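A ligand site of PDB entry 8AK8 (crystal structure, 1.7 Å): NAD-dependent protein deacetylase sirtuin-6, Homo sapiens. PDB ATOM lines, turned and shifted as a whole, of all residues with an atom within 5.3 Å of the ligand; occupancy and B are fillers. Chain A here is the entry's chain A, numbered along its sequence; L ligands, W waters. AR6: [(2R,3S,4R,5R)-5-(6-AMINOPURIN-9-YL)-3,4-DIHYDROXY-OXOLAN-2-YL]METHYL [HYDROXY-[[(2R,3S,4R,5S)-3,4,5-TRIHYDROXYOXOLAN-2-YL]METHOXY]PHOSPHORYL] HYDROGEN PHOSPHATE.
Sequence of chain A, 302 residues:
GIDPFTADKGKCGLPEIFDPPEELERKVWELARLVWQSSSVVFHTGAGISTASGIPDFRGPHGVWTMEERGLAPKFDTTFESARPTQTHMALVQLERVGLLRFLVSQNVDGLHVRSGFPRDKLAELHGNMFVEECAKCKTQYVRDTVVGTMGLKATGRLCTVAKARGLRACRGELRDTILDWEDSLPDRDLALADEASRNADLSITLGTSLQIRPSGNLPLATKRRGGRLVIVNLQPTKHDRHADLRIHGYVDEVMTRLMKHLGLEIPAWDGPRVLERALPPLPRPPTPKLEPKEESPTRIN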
ATOM      1  N   GLU A  16      11.585   3.928 -22.914  1.00  0.00           N
ATOM      2  CA  GLU A  16      10.642   2.926 -23.479  1.00  0.00           C
ATOM      3  C   GLU A  16      10.929   2.760 -24.957  1.00  0.00           C
ATOM      4  O   GLU A  16      11.455   3.682 -25.622  1.00  0.00           O
ATOM      5  CB  GLU A  16       9.202   3.353 -23.198  1.00  0.00           C
ATOM      6  CG  GLU A  16       8.915   3.448 -21.726  1.00  0.00           C
ATOM      7  CD  GLU A  16       7.476   3.774 -21.432  1.00  0.00           C
ATOM      8  OE1 GLU A  16       6.908   4.589 -22.191  1.00  0.00           O
ATOM      9  OE2 GLU A  16       6.943   3.219 -20.454  1.00  0.00           O
ATOM     10  N   THR A  45       5.374 -12.975 -14.981  1.00  0.00           N
ATOM     11  CA  THR A  45       4.750 -11.630 -14.929  1.00  0.00           C
ATOM     12  C   THR A  45       5.428 -10.777 -13.851  1.00  0.00           C
ATOM     13  O   THR A  45       5.789 -11.297 -12.741  1.00  0.00           O
ATOM     14  CB  THR A  45       3.239 -11.682 -14.685  1.00  0.00           C
ATOM     15  OG1 THR A  45       2.950 -12.194 -13.385  1.00  0.00           O
ATOM     16  CG2 THR A  45       2.483 -12.500 -15.702  1.00  0.00           C
ATOM     17  N   GLY A  46       5.573  -9.496 -14.140  1.00  0.00           N
ATOM     18  CA  GLY A  46       5.942  -8.514 -13.134  1.00  0.00           C
ATOM     19  C   GLY A  46       5.073  -7.279 -13.226  1.00  0.00           C
ATOM     20  O   GLY A  46       3.960  -7.352 -13.803  1.00  0.00           O
ATOM     21  N   ALA A  47       5.589  -6.215 -12.619  1.00  0.00           N
ATOM     22  CA  ALA A  47       4.760  -5.056 -12.205  1.00  0.00           C
ATOM     23  C   ALA A  47       4.109  -4.447 -13.450  1.00  0.00           C
ATOM     24  O   ALA A  47       2.993  -3.858 -13.314  1.00  0.00           O
ATOM     25  CB  ALA A  47       5.543  -4.063 -11.388  1.00  0.00           C
ATOM     26  N   GLY A  48       4.734  -4.564 -14.635  1.00  0.00           N
ATOM     27  CA  GLY A  48       4.210  -3.969 -15.892  1.00  0.00           C
ATOM     28  C   GLY A  48       2.800  -4.475 -16.251  1.00  0.00           C
ATOM     29  O   GLY A  48       2.049  -3.750 -16.952  1.00  0.00           O
ATOM     30  N   ILE A  49       2.393  -5.655 -15.793  1.00  0.00           N
ATOM     31  CA  ILE A  49       1.026  -6.165 -16.146  1.00  0.00           C
ATOM     32  C   ILE A  49      -0.066  -5.518 -15.277  1.00  0.00           C
ATOM     33  O   ILE A  49      -1.217  -5.886 -15.454  1.00  0.00           O
ATOM     34  CB  ILE A  49       0.932  -7.706 -16.157  1.00  0.00           C
ATOM     35  CG1 ILE A  49       0.867  -8.308 -14.758  1.00  0.00           C
ATOM     36  CG2 ILE A  49       2.048  -8.314 -16.983  1.00  0.00           C
ATOM     37  CD1 ILE A  49       0.112  -9.631 -14.722  1.00  0.00           C
ATOM     38  N   THR A  51       0.107  -1.928 -14.357  1.00  0.00           N
ATOM     39  CA  THR A  51       0.176  -0.464 -14.588  1.00  0.00           C
ATOM     40  C   THR A  51      -1.159  -0.006 -15.159  1.00  0.00           C
ATOM     41  O   THR A  51      -1.613   1.086 -14.742  1.00  0.00           O
ATOM     42  CB  THR A  51       1.392  -0.058 -15.413  1.00  0.00           C
ATOM     43  OG1 THR A  51       1.356  -0.748 -16.651  1.00  0.00           O
ATOM     44  CG2 THR A  51       2.721  -0.260 -14.686  1.00  0.00           C
ATOM     45  N   ALA A  52      -1.777  -0.772 -16.064  1.00  0.00           N
ATOM     46  CA  ALA A  52      -3.101  -0.418 -16.705  1.00  0.00           C
ATOM     47  C   ALA A  52      -4.297  -0.543 -15.744  1.00  0.00           C
ATOM     48  O   ALA A  52      -5.400  -0.078 -16.110  1.00  0.00           O
ATOM     49  CB  ALA A  52      -3.306  -1.227 -17.941  1.00  0.00           C
ATOM     50  N   ASP A  57       4.568   0.648 -11.628  1.00  0.00           N
ATOM     51  CA  ASP A  57       5.634  -0.395 -11.574  1.00  0.00           C
ATOM     52  C   ASP A  57       6.789   0.150 -10.718  1.00  0.00           C
ATOM     53  O   ASP A  57       6.590   1.115  -9.953  1.00  0.00           O
ATOM     54  CB  ASP A  57       6.017  -0.842 -12.974  1.00  0.00           C
ATOM     55  CG  ASP A  57       6.604   0.240 -13.870  1.00  0.00           C
ATOM     56  OD1 ASP A  57       7.068   1.273 -13.329  1.00  0.00           O
ATOM     57  OD2 ASP A  57       6.600   0.019 -15.084  1.00  0.00           O
ATOM     58  N   PHE A  58       7.939  -0.544 -10.728  1.00  0.00           N
ATOM     59  CA  PHE A  58       9.121  -0.178  -9.924  1.00  0.00           C
ATOM     60  C   PHE A  58      10.123   0.663 -10.734  1.00  0.00           C
ATOM     61  O   PHE A  58      10.750   1.597 -10.127  1.00  0.00           O
ATOM     62  CB  PHE A  58       9.761  -1.448  -9.368  1.00  0.00           C
ATOM     63  CG  PHE A  58       8.904  -2.081  -8.328  1.00  0.00           C
ATOM     64  CD1 PHE A  58       8.951  -1.635  -7.019  1.00  0.00           C
ATOM     65  CD2 PHE A  58       8.012  -3.088  -8.665  1.00  0.00           C
ATOM     66  CE1 PHE A  58       8.115  -2.183  -6.067  1.00  0.00           C
ATOM     67  CE2 PHE A  58       7.189  -3.646  -7.697  1.00  0.00           C
ATOM     68  CZ  PHE A  58       7.251  -3.196  -6.405  1.00  0.00           C
ATOM     69  N   ARG A  59      10.363   0.301 -11.997  1.00  0.00           N
ATOM     70  CA  ARG A  59      11.581   0.701 -12.748  1.00  0.00           C
ATOM     71  C   ARG A  59      11.211   1.324 -14.091  1.00  0.00           C
ATOM     72  O   ARG A  59      12.137   1.811 -14.800  1.00  0.00           O
ATOM     73  CB  ARG A  59      12.536  -0.482 -12.957  1.00  0.00           C
ATOM     74  CG  ARG A  59      13.131  -0.920 -11.628  1.00  0.00           C
ATOM     75  CD  ARG A  59      14.159  -2.013 -11.737  1.00  0.00           C
ATOM     76  NE  ARG A  59      14.460  -2.543 -10.426  1.00  0.00           N
ATOM     77  CZ  ARG A  59      13.756  -3.452  -9.751  1.00  0.00           C
ATOM     78  NH1 ARG A  59      12.645  -3.987 -10.246  1.00  0.00           N
ATOM     79  NH2 ARG A  59      14.160  -3.812  -8.543  1.00  0.00           N
ATOM     80  N   GLY A  60       9.908   1.496 -14.337  1.00  0.00           N
ATOM     81  CA  GLY A  60       9.413   2.250 -15.503  1.00  0.00           C
ATOM     82  C   GLY A  60       9.601   3.765 -15.328  1.00  0.00           C
ATOM     83  O   GLY A  60      10.005   4.239 -14.278  1.00  0.00           O
ATOM     84  N   TRP A  65      10.782   2.971  -7.743  1.00  0.00           N
ATOM     85  CA  TRP A  65      12.237   3.196  -7.542  1.00  0.00           C
ATOM     86  C   TRP A  65      12.725   4.356  -8.422  1.00  0.00           C
ATOM     87  O   TRP A  65      13.536   5.191  -7.937  1.00  0.00           O
ATOM     88  CB  TRP A  65      13.076   1.945  -7.787  1.00  0.00           C
ATOM     89  CG  TRP A  65      12.702   0.722  -7.005  1.00  0.00           C
ATOM     90  CD1 TRP A  65      12.863  -0.556  -7.443  1.00  0.00           C
ATOM     91  CD2 TRP A  65      12.160   0.621  -5.671  1.00  0.00           C
ATOM     92  NE1 TRP A  65      12.450  -1.435  -6.493  1.00  0.00           N
ATOM     93  CE2 TRP A  65      12.025  -0.750  -5.389  1.00  0.00           C
ATOM     94  CE3 TRP A  65      11.815   1.539  -4.668  1.00  0.00           C
ATOM     95  CZ2 TRP A  65      11.509  -1.231  -4.188  1.00  0.00           C
ATOM     96  CZ3 TRP A  65      11.301   1.071  -3.474  1.00  0.00           C
ATOM     97  CH2 TRP A  65      11.157  -0.301  -3.238  1.00  0.00           C
ATOM     98  N   GLN A 107       6.358 -12.139  -9.854  1.00  0.00           N
ATOM     99  CA  GLN A 107       7.059 -11.301  -8.875  1.00  0.00           C
ATOM    100  C   GLN A 107       6.076 -10.336  -8.208  1.00  0.00           C
ATOM    101  O   GLN A 107       6.481  -9.649  -7.317  1.00  0.00           O
ATOM    102  CB  GLN A 107       8.183 -10.586  -9.607  1.00  0.00           C
ATOM    103  CG  GLN A 107       9.213 -11.542 -10.217  1.00  0.00           C
ATOM    104  CD  GLN A 107      10.147 -10.803 -11.132  1.00  0.00           C
ATOM    105  OE1 GLN A 107      10.975 -10.025 -10.652  1.00  0.00           O
ATOM    106  NE2 GLN A 107      10.030 -11.070 -12.429  1.00  0.00           N
ATOM    107  N   ASN A 108       4.833 -10.255  -8.667  1.00  0.00           N
ATOM    108  CA  ASN A 108       3.883  -9.236  -8.177  1.00  0.00           C
ATOM    109  C   ASN A 108       3.366  -9.613  -6.779  1.00  0.00           C
ATOM    110  O   ASN A 108       3.002 -10.792  -6.539  1.00  0.00           O
ATOM    111  CB  ASN A 108       2.762  -9.026  -9.185  1.00  0.00           C
ATOM    112  CG  ASN A 108       3.292  -8.429 -10.480  1.00  0.00           C
ATOM    113  OD1 ASN A 108       4.432  -7.962 -10.568  1.00  0.00           O
ATOM    114  ND2 ASN A 108       2.476  -8.517 -11.515  1.00  0.00           N
ATOM    115  N   HIS A 127       7.395 -13.289  -4.573  1.00  0.00           N
ATOM    116  CA  HIS A 127       7.714 -12.147  -3.664  1.00  0.00           C
ATOM    117  C   HIS A 127       6.618 -11.975  -2.612  1.00  0.00           C
ATOM    118  O   HIS A 127       6.721 -11.068  -1.755  1.00  0.00           O
ATOM    119  CB  HIS A 127       8.003 -10.874  -4.485  1.00  0.00           C
ATOM    120  CG  HIS A 127       9.165 -11.028  -5.407  1.00  0.00           C
ATOM    121  ND1 HIS A 127       9.494 -10.094  -6.387  1.00  0.00           N
ATOM    122  CD2 HIS A 127      10.085 -12.018  -5.489  1.00  0.00           C
ATOM    123  CE1 HIS A 127      10.529 -10.524  -7.070  1.00  0.00           C
ATOM    124  NE2 HIS A 127      10.968 -11.688  -6.497  1.00  0.00           N
ATOM    125  N   TRP A 182      14.071  -7.202   1.592  1.00  0.00           N
ATOM    126  CA  TRP A 182      15.291  -7.335   0.765  1.00  0.00           C
ATOM    127  C   TRP A 182      16.115  -8.567   1.177  1.00  0.00           C
ATOM    128  O   TRP A 182      16.600  -9.281   0.291  1.00  0.00           O
ATOM    129  CB  TRP A 182      16.124  -6.043   0.852  1.00  0.00           C
ATOM    130  CG  TRP A 182      15.470  -4.884   0.164  1.00  0.00           C
ATOM    131  CD1 TRP A 182      14.777  -3.862   0.752  1.00  0.00           C
ATOM    132  CD2 TRP A 182      15.417  -4.641  -1.253  1.00  0.00           C
ATOM    133  NE1 TRP A 182      14.307  -2.993  -0.205  1.00  0.00           N
ATOM    134  CE2 TRP A 182      14.678  -3.455  -1.442  1.00  0.00           C
ATOM    135  CE3 TRP A 182      15.915  -5.316  -2.375  1.00  0.00           C
ATOM    136  CZ2 TRP A 182      14.437  -2.924  -2.705  1.00  0.00           C
ATOM    137  CZ3 TRP A 182      15.667  -4.785  -3.626  1.00  0.00           C
ATOM    138  CH2 TRP A 182      14.935  -3.608  -3.786  1.00  0.00           C
ATOM    139  N   GLY A 208       5.781  -7.604 -18.822  1.00  0.00           N
ATOM    140  CA  GLY A 208       5.985  -6.463 -17.894  1.00  0.00           C
ATOM    141  C   GLY A 208       6.867  -6.779 -16.705  1.00  0.00           C
ATOM    142  O   GLY A 208       6.480  -6.395 -15.642  1.00  0.00           O
ATOM    143  N   THR A 209       8.032  -7.396 -16.926  1.00  0.00           N
ATOM    144  CA  THR A 209       9.138  -7.534 -15.969  1.00  0.00           C
ATOM    145  C   THR A 209      10.471  -7.179 -16.664  1.00  0.00           C
ATOM    146  O   THR A 209      10.736  -7.687 -17.788  1.00  0.00           O
ATOM    147  CB  THR A 209       9.216  -8.944 -15.371  1.00  0.00           C
ATOM    148  OG1 THR A 209      10.333  -8.800 -14.498  1.00  0.00           O
ATOM    149  CG2 THR A 209       9.370 -10.044 -16.413  1.00  0.00           C
ATOM    150  N   SER A 210      11.265  -6.355 -15.996  1.00  0.00           N
ATOM    151  CA  SER A 210      12.632  -5.950 -16.434  1.00  0.00           C
ATOM    152  C   SER A 210      13.642  -7.092 -16.174  1.00  0.00           C
ATOM    153  O   SER A 210      14.793  -6.958 -16.654  1.00  0.00           O
ATOM    154  CB  SER A 210      13.047  -4.651 -15.760  1.00  0.00           C
ATOM    155  OG  SER A 210      13.258  -4.824 -14.374  1.00  0.00           O
ATOM    156  N   LEU A 211      13.237  -8.138 -15.455  1.00  0.00           N
ATOM    157  CA  LEU A 211      14.040  -9.400 -15.220  1.00  0.00           C
ATOM    158  C   LEU A 211      15.366  -9.095 -14.474  1.00  0.00           C
ATOM    159  O   LEU A 211      16.373  -9.814 -14.704  1.00  0.00           O
ATOM    160  CB  LEU A 211      14.316 -10.102 -16.548  1.00  0.00           C
ATOM    161  CG  LEU A 211      13.090 -10.506 -17.359  1.00  0.00           C
ATOM    162  CD1 LEU A 211      13.464 -10.962 -18.763  1.00  0.00           C
ATOM    163  CD2 LEU A 211      12.288 -11.555 -16.611  1.00  0.00           C
ATOM    164  N   GLN A 212      15.370  -8.116 -13.584  1.00  0.00           N
ATOM    165  CA  GLN A 212      16.605  -7.602 -12.933  1.00  0.00           C
ATOM    166  C   GLN A 212      16.832  -8.290 -11.576  1.00  0.00           C
ATOM    167  O   GLN A 212      17.935  -8.120 -11.007  1.00  0.00           O
ATOM    168  CB  GLN A 212      16.533  -6.084 -12.777  1.00  0.00           C
ATOM    169  CG  GLN A 212      16.438  -5.326 -14.090  1.00  0.00           C
ATOM    170  CD  GLN A 212      16.733  -3.858 -13.905  1.00  0.00           C
ATOM    171  OE1 GLN A 212      17.656  -3.502 -13.182  1.00  0.00           O
ATOM    172  NE2 GLN A 212      15.963  -2.984 -14.572  1.00  0.00           N
ATOM    173  N   ILE A 213      15.815  -8.977 -11.028  1.00  0.00           N
ATOM    174  CA  ILE A 213      15.851  -9.573  -9.672  1.00  0.00           C
ATOM    175  C   ILE A 213      16.201 -11.043  -9.818  1.00  0.00           C
ATOM    176  O   ILE A 213      15.517 -11.734 -10.592  1.00  0.00           O
ATOM    177  CB  ILE A 213      14.510  -9.380  -8.920  1.00  0.00           C
ATOM    178  CG1 ILE A 213      14.248  -7.898  -8.632  1.00  0.00           C
ATOM    179  CG2 ILE A 213      14.478 -10.221  -7.655  1.00  0.00           C
ATOM    180  CD1 ILE A 213      15.298  -7.238  -7.756  1.00  0.00           C
ATOM    181  N   VAL A 233       8.023  -9.690 -23.517  1.00  0.00           N
ATOM    182  CA  VAL A 233       7.083  -8.581 -23.851  1.00  0.00           C
ATOM    183  C   VAL A 233       7.333  -7.526 -22.776  1.00  0.00           C
ATOM    184  O   VAL A 233       7.131  -7.812 -21.574  1.00  0.00           O
ATOM    185  CB  VAL A 233       5.624  -9.067 -23.877  1.00  0.00           C
ATOM    186  CG1 VAL A 233       4.688  -7.924 -24.290  1.00  0.00           C
ATOM    187  CG2 VAL A 233       5.377 -10.279 -24.768  1.00  0.00           C
ATOM    188  N   ASN A 234       7.794  -6.339 -23.165  1.00  0.00           N
ATOM    189  CA  ASN A 234       8.200  -5.272 -22.215  1.00  0.00           C
ATOM    190  C   ASN A 234       8.438  -3.979 -22.993  1.00  0.00           C
ATOM    191  O   ASN A 234       9.045  -4.057 -24.093  1.00  0.00           O
ATOM    192  CB  ASN A 234       9.461  -5.678 -21.430  1.00  0.00           C
ATOM    193  CG  ASN A 234       9.475  -5.052 -20.057  1.00  0.00           C
ATOM    194  OD1 ASN A 234       8.557  -5.264 -19.264  1.00  0.00           O
ATOM    195  ND2 ASN A 234      10.459  -4.214 -19.776  1.00  0.00           N
ATOM    196  N   LEU A 235       7.997  -2.853 -22.435  1.00  0.00           N
ATOM    197  CA  LEU A 235       8.179  -1.509 -23.035  1.00  0.00           C
ATOM    198  C   LEU A 235       9.662  -1.090 -22.962  1.00  0.00           C
ATOM    199  O   LEU A 235      10.153  -0.457 -23.933  1.00  0.00           O
ATOM    200  CB  LEU A 235       7.267  -0.523 -22.298  1.00  0.00           C
ATOM    201  CG  LEU A 235       5.804  -0.577 -22.702  1.00  0.00           C
ATOM    202  CD1 LEU A 235       4.982   0.279 -21.752  1.00  0.00           C
ATOM    203  CD2 LEU A 235       5.646  -0.131 -24.174  1.00  0.00           C
ATOM    204  N   GLN A 236      10.344  -1.446 -21.870  1.00  0.00           N
ATOM    205  CA  GLN A 236      11.773  -1.076 -21.632  1.00  0.00           C
ATOM    206  C   GLN A 236      12.633  -2.276 -21.980  1.00  0.00           C
ATOM    207  O   GLN A 236      12.124  -3.389 -22.116  1.00  0.00           O
ATOM    208  CB  GLN A 236      12.050  -0.730 -20.172  1.00  0.00           C
ATOM    209  CG  GLN A 236      11.521   0.617 -19.717  1.00  0.00           C
ATOM    210  CD  GLN A 236      11.734   0.819 -18.222  1.00  0.00           C
ATOM    211  OE1 GLN A 236      11.607  -0.087 -17.383  1.00  0.00           O
ATOM    212  NE2 GLN A 236      12.049   2.038 -17.848  1.00  0.00           N
ATOM    213  N   PRO A 237      13.961  -2.071 -22.167  1.00  0.00           N
ATOM    214  CA  PRO A 237      14.915  -3.167 -22.123  1.00  0.00           C
ATOM    215  C   PRO A 237      14.801  -3.985 -20.847  1.00  0.00           C
ATOM    216  O   PRO A 237      14.488  -3.449 -19.815  1.00  0.00           O
ATOM    217  CB  PRO A 237      16.288  -2.458 -22.144  1.00  0.00           C
ATOM    218  CG  PRO A 237      15.995  -1.128 -22.813  1.00  0.00           C
ATOM    219  CD  PRO A 237      14.606  -0.767 -22.350  1.00  0.00           C
ATOM    220  N   GLY A 250       5.648  -3.211 -26.679  1.00  0.00           N
ATOM    221  CA  GLY A 250       4.278  -2.658 -26.775  1.00  0.00           C
ATOM    222  C   GLY A 250       3.545  -2.807 -25.452  1.00  0.00           C
ATOM    223  O   GLY A 250       4.064  -3.469 -24.541  1.00  0.00           O
ATOM    224  N   TYR A 251       2.376  -2.230 -25.312  1.00  0.00           N
ATOM    225  CA  TYR A 251       1.542  -2.427 -24.098  1.00  0.00           C
ATOM    226  C   TYR A 251       1.114  -3.895 -23.994  1.00  0.00           C
ATOM    227  O   TYR A 251       0.684  -4.502 -25.021  1.00  0.00           O
ATOM    228  CB  TYR A 251       0.390  -1.429 -24.101  1.00  0.00           C
ATOM    229  CG  TYR A 251       0.860  -0.011 -23.972  1.00  0.00           C
ATOM    230  CD1 TYR A 251       1.184   0.537 -22.742  1.00  0.00           C
ATOM    231  CD2 TYR A 251       1.008   0.778 -25.108  1.00  0.00           C
ATOM    232  CE1 TYR A 251       1.588   1.846 -22.621  1.00  0.00           C
ATOM    233  CE2 TYR A 251       1.468   2.081 -25.004  1.00  0.00           C
ATOM    234  CZ  TYR A 251       1.747   2.614 -23.759  1.00  0.00           C
ATOM    235  OH  TYR A 251       2.189   3.906 -23.680  1.00  0.00           O
ATOM    236  N   VAL A 252       1.281  -4.493 -22.809  1.00  0.00           N
ATOM    237  CA  VAL A 252       1.020  -5.931 -22.632  1.00  0.00           C
ATOM    238  C   VAL A 252      -0.464  -6.217 -22.887  1.00  0.00           C
ATOM    239  O   VAL A 252      -0.727  -7.200 -23.546  1.00  0.00           O
ATOM    240  CB  VAL A 252       1.580  -6.467 -21.310  1.00  0.00           C
ATOM    241  CG1 VAL A 252       0.878  -5.932 -20.053  1.00  0.00           C
ATOM    242  CG2 VAL A 252       1.607  -7.976 -21.371  1.00  0.00           C
ATOM    243  N   ASP A 253      -1.389  -5.279 -22.645  1.00  0.00           N
ATOM    244  CA  ASP A 253      -2.836  -5.480 -22.955  1.00  0.00           C
ATOM    245  C   ASP A 253      -3.073  -5.551 -24.475  1.00  0.00           C
ATOM    246  O   ASP A 253      -3.930  -6.376 -24.888  1.00  0.00           O
ATOM    247  CB  ASP A 253      -3.710  -4.400 -22.313  1.00  0.00           C
ATOM    248  CG  ASP A 253      -3.993  -4.572 -20.838  1.00  0.00           C
ATOM    249  OD1 ASP A 253      -3.659  -5.684 -20.267  1.00  0.00           O
ATOM    250  OD2 ASP A 253      -4.464  -3.561 -20.243  1.00  0.00           O
HETATM  251  N1  AR6 L   1       2.992  -2.956 -21.041  1.00  0.00           N
HETATM  252  C2  AR6 L   1       4.223  -3.444 -21.183  1.00  0.00           C
HETATM  253  N3  AR6 L   1       5.301  -3.262 -20.396  1.00  0.00           N
HETATM  254  C4  AR6 L   1       5.007  -2.495 -19.337  1.00  0.00           C
HETATM  255  C5  AR6 L   1       3.785  -1.919 -19.049  1.00  0.00           C
HETATM  256  C6  AR6 L   1       2.729  -2.186 -19.941  1.00  0.00           C
HETATM  257  N6  AR6 L   1       1.496  -1.710 -19.791  1.00  0.00           N
HETATM  258  N7  AR6 L   1       3.868  -1.204 -17.866  1.00  0.00           N
HETATM  259  C8  AR6 L   1       5.118  -1.311 -17.475  1.00  0.00           C
HETATM  260  N9  AR6 L   1       5.851  -2.085 -18.330  1.00  0.00           N
HETATM  261  PA  AR6 L   1       9.985  -3.485 -13.051  1.00  0.00           P
HETATM  262  PB  AR6 L   1       9.421  -6.125 -11.871  1.00  0.00           P
HETATM  263  C1' AR6 L   1       7.216  -2.508 -18.147  1.00  0.00           C
HETATM  264  O1A AR6 L   1      11.436  -3.642 -12.791  1.00  0.00           O
HETATM  265  O1B AR6 L   1       8.114  -6.776 -11.544  1.00  0.00           O
HETATM  266  C1D AR6 L   1      11.063  -4.910  -7.080  1.00  0.00           C
HETATM  267  O1D AR6 L   1      11.985  -4.503  -6.096  1.00  0.00           O
HETATM  268  C2' AR6 L   1       8.232  -1.478 -17.679  1.00  0.00           C
HETATM  269  O2' AR6 L   1       8.859  -1.029 -18.844  1.00  0.00           O
HETATM  270  O2A AR6 L   1       9.261  -2.217 -12.730  1.00  0.00           O
HETATM  271  O2B AR6 L   1      10.247  -6.687 -12.958  1.00  0.00           O
HETATM  272  C2D AR6 L   1       9.933  -5.799  -6.514  1.00  0.00           C
HETATM  273  O2D AR6 L   1      10.334  -6.699  -5.505  1.00  0.00           O
HETATM  274  C3' AR6 L   1       9.187  -2.300 -16.802  1.00  0.00           C
HETATM  275  O3' AR6 L   1      10.385  -2.569 -17.476  1.00  0.00           O
HETATM  276  O3A AR6 L   1       9.149  -4.575 -12.216  1.00  0.00           O
HETATM  277  C3D AR6 L   1       9.476  -6.567  -7.758  1.00  0.00           C
HETATM  278  O3D AR6 L   1       8.711  -7.744  -7.444  1.00  0.00           O
HETATM  279  C4' AR6 L   1       8.466  -3.635 -16.555  1.00  0.00           C
HETATM  280  O4' AR6 L   1       7.152  -3.459 -17.128  1.00  0.00           O
HETATM  281  C4D AR6 L   1      10.820  -6.870  -8.400  1.00  0.00           C
HETATM  282  O4D AR6 L   1      11.655  -5.705  -8.123  1.00  0.00           O
HETATM  283  C5' AR6 L   1       8.359  -3.896 -15.078  1.00  0.00           C
HETATM  284  O5' AR6 L   1       9.708  -3.856 -14.566  1.00  0.00           O
HETATM  285  C5D AR6 L   1      10.786  -7.116  -9.886  1.00  0.00           C
HETATM  286  O5D AR6 L   1      10.258  -5.908 -10.564  1.00  0.00           O
HETATM  287  O   HOH W   1       7.759   1.317 -19.067  1.00  0.00           O
HETATM  288  O   HOH W   2      13.116  -6.501 -12.617  1.00  0.00           O
HETATM  289  O   HOH W   3      -0.532  -2.948 -17.551  1.00  0.00           O
HETATM  290  O   HOH W   4      -1.010  -3.087 -20.698  1.00  0.00           O
HETATM  291  O   HOH W   5       6.731  -7.185  -9.373  1.00  0.00           O
HETATM  292  O   HOH W   6       8.381  -7.150  -3.862  1.00  0.00           O
HETATM  293  O   HOH W   7       6.021  -6.985  -6.086  1.00  0.00           O
HETATM  294  O   HOH W   8       6.119   1.861 -16.827  1.00  0.00           O
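O2B of the ligand sits at hydrogen-bond distance from OG1 of Thr 209 (2.6 Å). An oxygen (O2B) of the ligand lies within hydrogen-bond range of the backbone NH (N) of Ser 210 (3.2 Å). OG of Ser 210 lies within hydrogen-bond range of O1A of the ligand (2.7 Å). O3D of the ligand sits at hydrogen-bond distance from ND1 of His 127. An oxygen (O2') of the ligand lies close to the backbone NH of Gln 236 (3.4 Å). OE1 of Gln 236 lies within hydrogen-bond range of O3' of the ligand, at 2.8 Å. N of Ala 47 is in hydrogen-bond range of O1B of the ligand (2.8 Å). OG1 of Thr 51 lies within hydrogen-bond range of N7 of the ligand, 2.8 Å away. O3' of the ligand lies within hydrogen-bond range of ND2 of Asn 234 (2.8 Å). The backbone NH (N) of Arg 59 is in hydrogen-bond range of an oxygen (O2A) of the ligand. The guanidinium group (NH1) of Arg 59 lies within salt-bridge range of an oxygen (O1A) of the ligand, 2.8 Å away. The backbone NH of Val 252 sits at hydrogen-bond distance from a nitrogen (N1) of the ligand. N of Phe 58 sits at hydrogen-bond distance from O2A of the ligand. The backbone carbonyl oxygen (O) of Gln 107 is in hydrogen-bond range of an oxygen (O3D) of the ligand. An oxygen (O1D) of the ligand sits at hydrogen-bond distance from the indole nitrogen (NE1) of Trp 65, at 3.1 Å. N of Leu 235 sits at hydrogen-bond distance from N3 of the ligand (3.4 Å).
The side-chain hydroxyl (OG1) of Thr 209 lies within hydrogen-bond range of the backbone NH (N) of Leu 211. The side-chain hydroxyl (OG) of Ser 210 sits close to the side-chain amide nitrogen (NE2) of Gln 212, at 3.3 Å. The backbone carbonyl oxygen (O) of Gln 236 lies within hydrogen-bond range of the side-chain amide nitrogen (ND2) of Asn 234 (3.0 Å). The backbone carbonyl oxygen of Gly 208 is in hydrogen-bond range of the backbone NH of Ala 47, at 3.2 Å. The side-chain hydroxyl (OG1) of Thr 51 sits at hydrogen-bond distance from the backbone carbonyl oxygen (O) of Gly 48, at 3.1 Å. The backbone carbonyl oxygen (O) of Phe 58 sits at hydrogen-bond distance from the backbone NH (N) of Trp 65 (2.8 Å). The backbone NH (N) of Gly 208 sits at hydrogen-bond distance from the backbone carbonyl oxygen (O) of Val 233 (3.1 Å). The side-chain amide nitrogen of Asn 108 is in hydrogen-bond range of the backbone carbonyl oxygen of Gly 46.
A nitrogen (N7) of the ligand lies close to the backbone carbonyl oxygen (O) of Gly 48 (3.3 Å). The backbone carbonyl oxygen (O) of Gly 208 sits close to an oxygen (O4') of the ligand (3.4 Å). Merely in contact with the ligand: Asp 57 (3.1 Å), Gly 46 (3.2 Å), Gly 250 (3.4 Å), Tyr 251 (3.4 Å), Ile 213 (3.4 Å), Trp 182 (3.9 Å) and Asn 108 (3.99 Å). Hydrophobic or aromatic side chains that line the ligand: Ala 47, Phe 58, Trp 65, His 127, Trp 182, Ile 213, Leu 235, Tyr 251 and Val 252. The nearest printed residue that does not touch the ligand is Gly 60 (4.1 Å).
Water W1 bridges OE2 of Glu 16 (2.5 Å) and O2' of the ligand (2.6 Å). Water W5 lies within hydrogen-bond range of O1B of the ligand, OD1 of Asn 108 and O of Gln 107. Water W7 lies within hydrogen-bond range of O of Gln 107 (3.0 Å) and O3D of the ligand (3.1 Å). Water W3 lies within hydrogen-bond range of O of Gly 48, N of Ala 52, OG1 of Thr 51 and N6 of the ligand.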
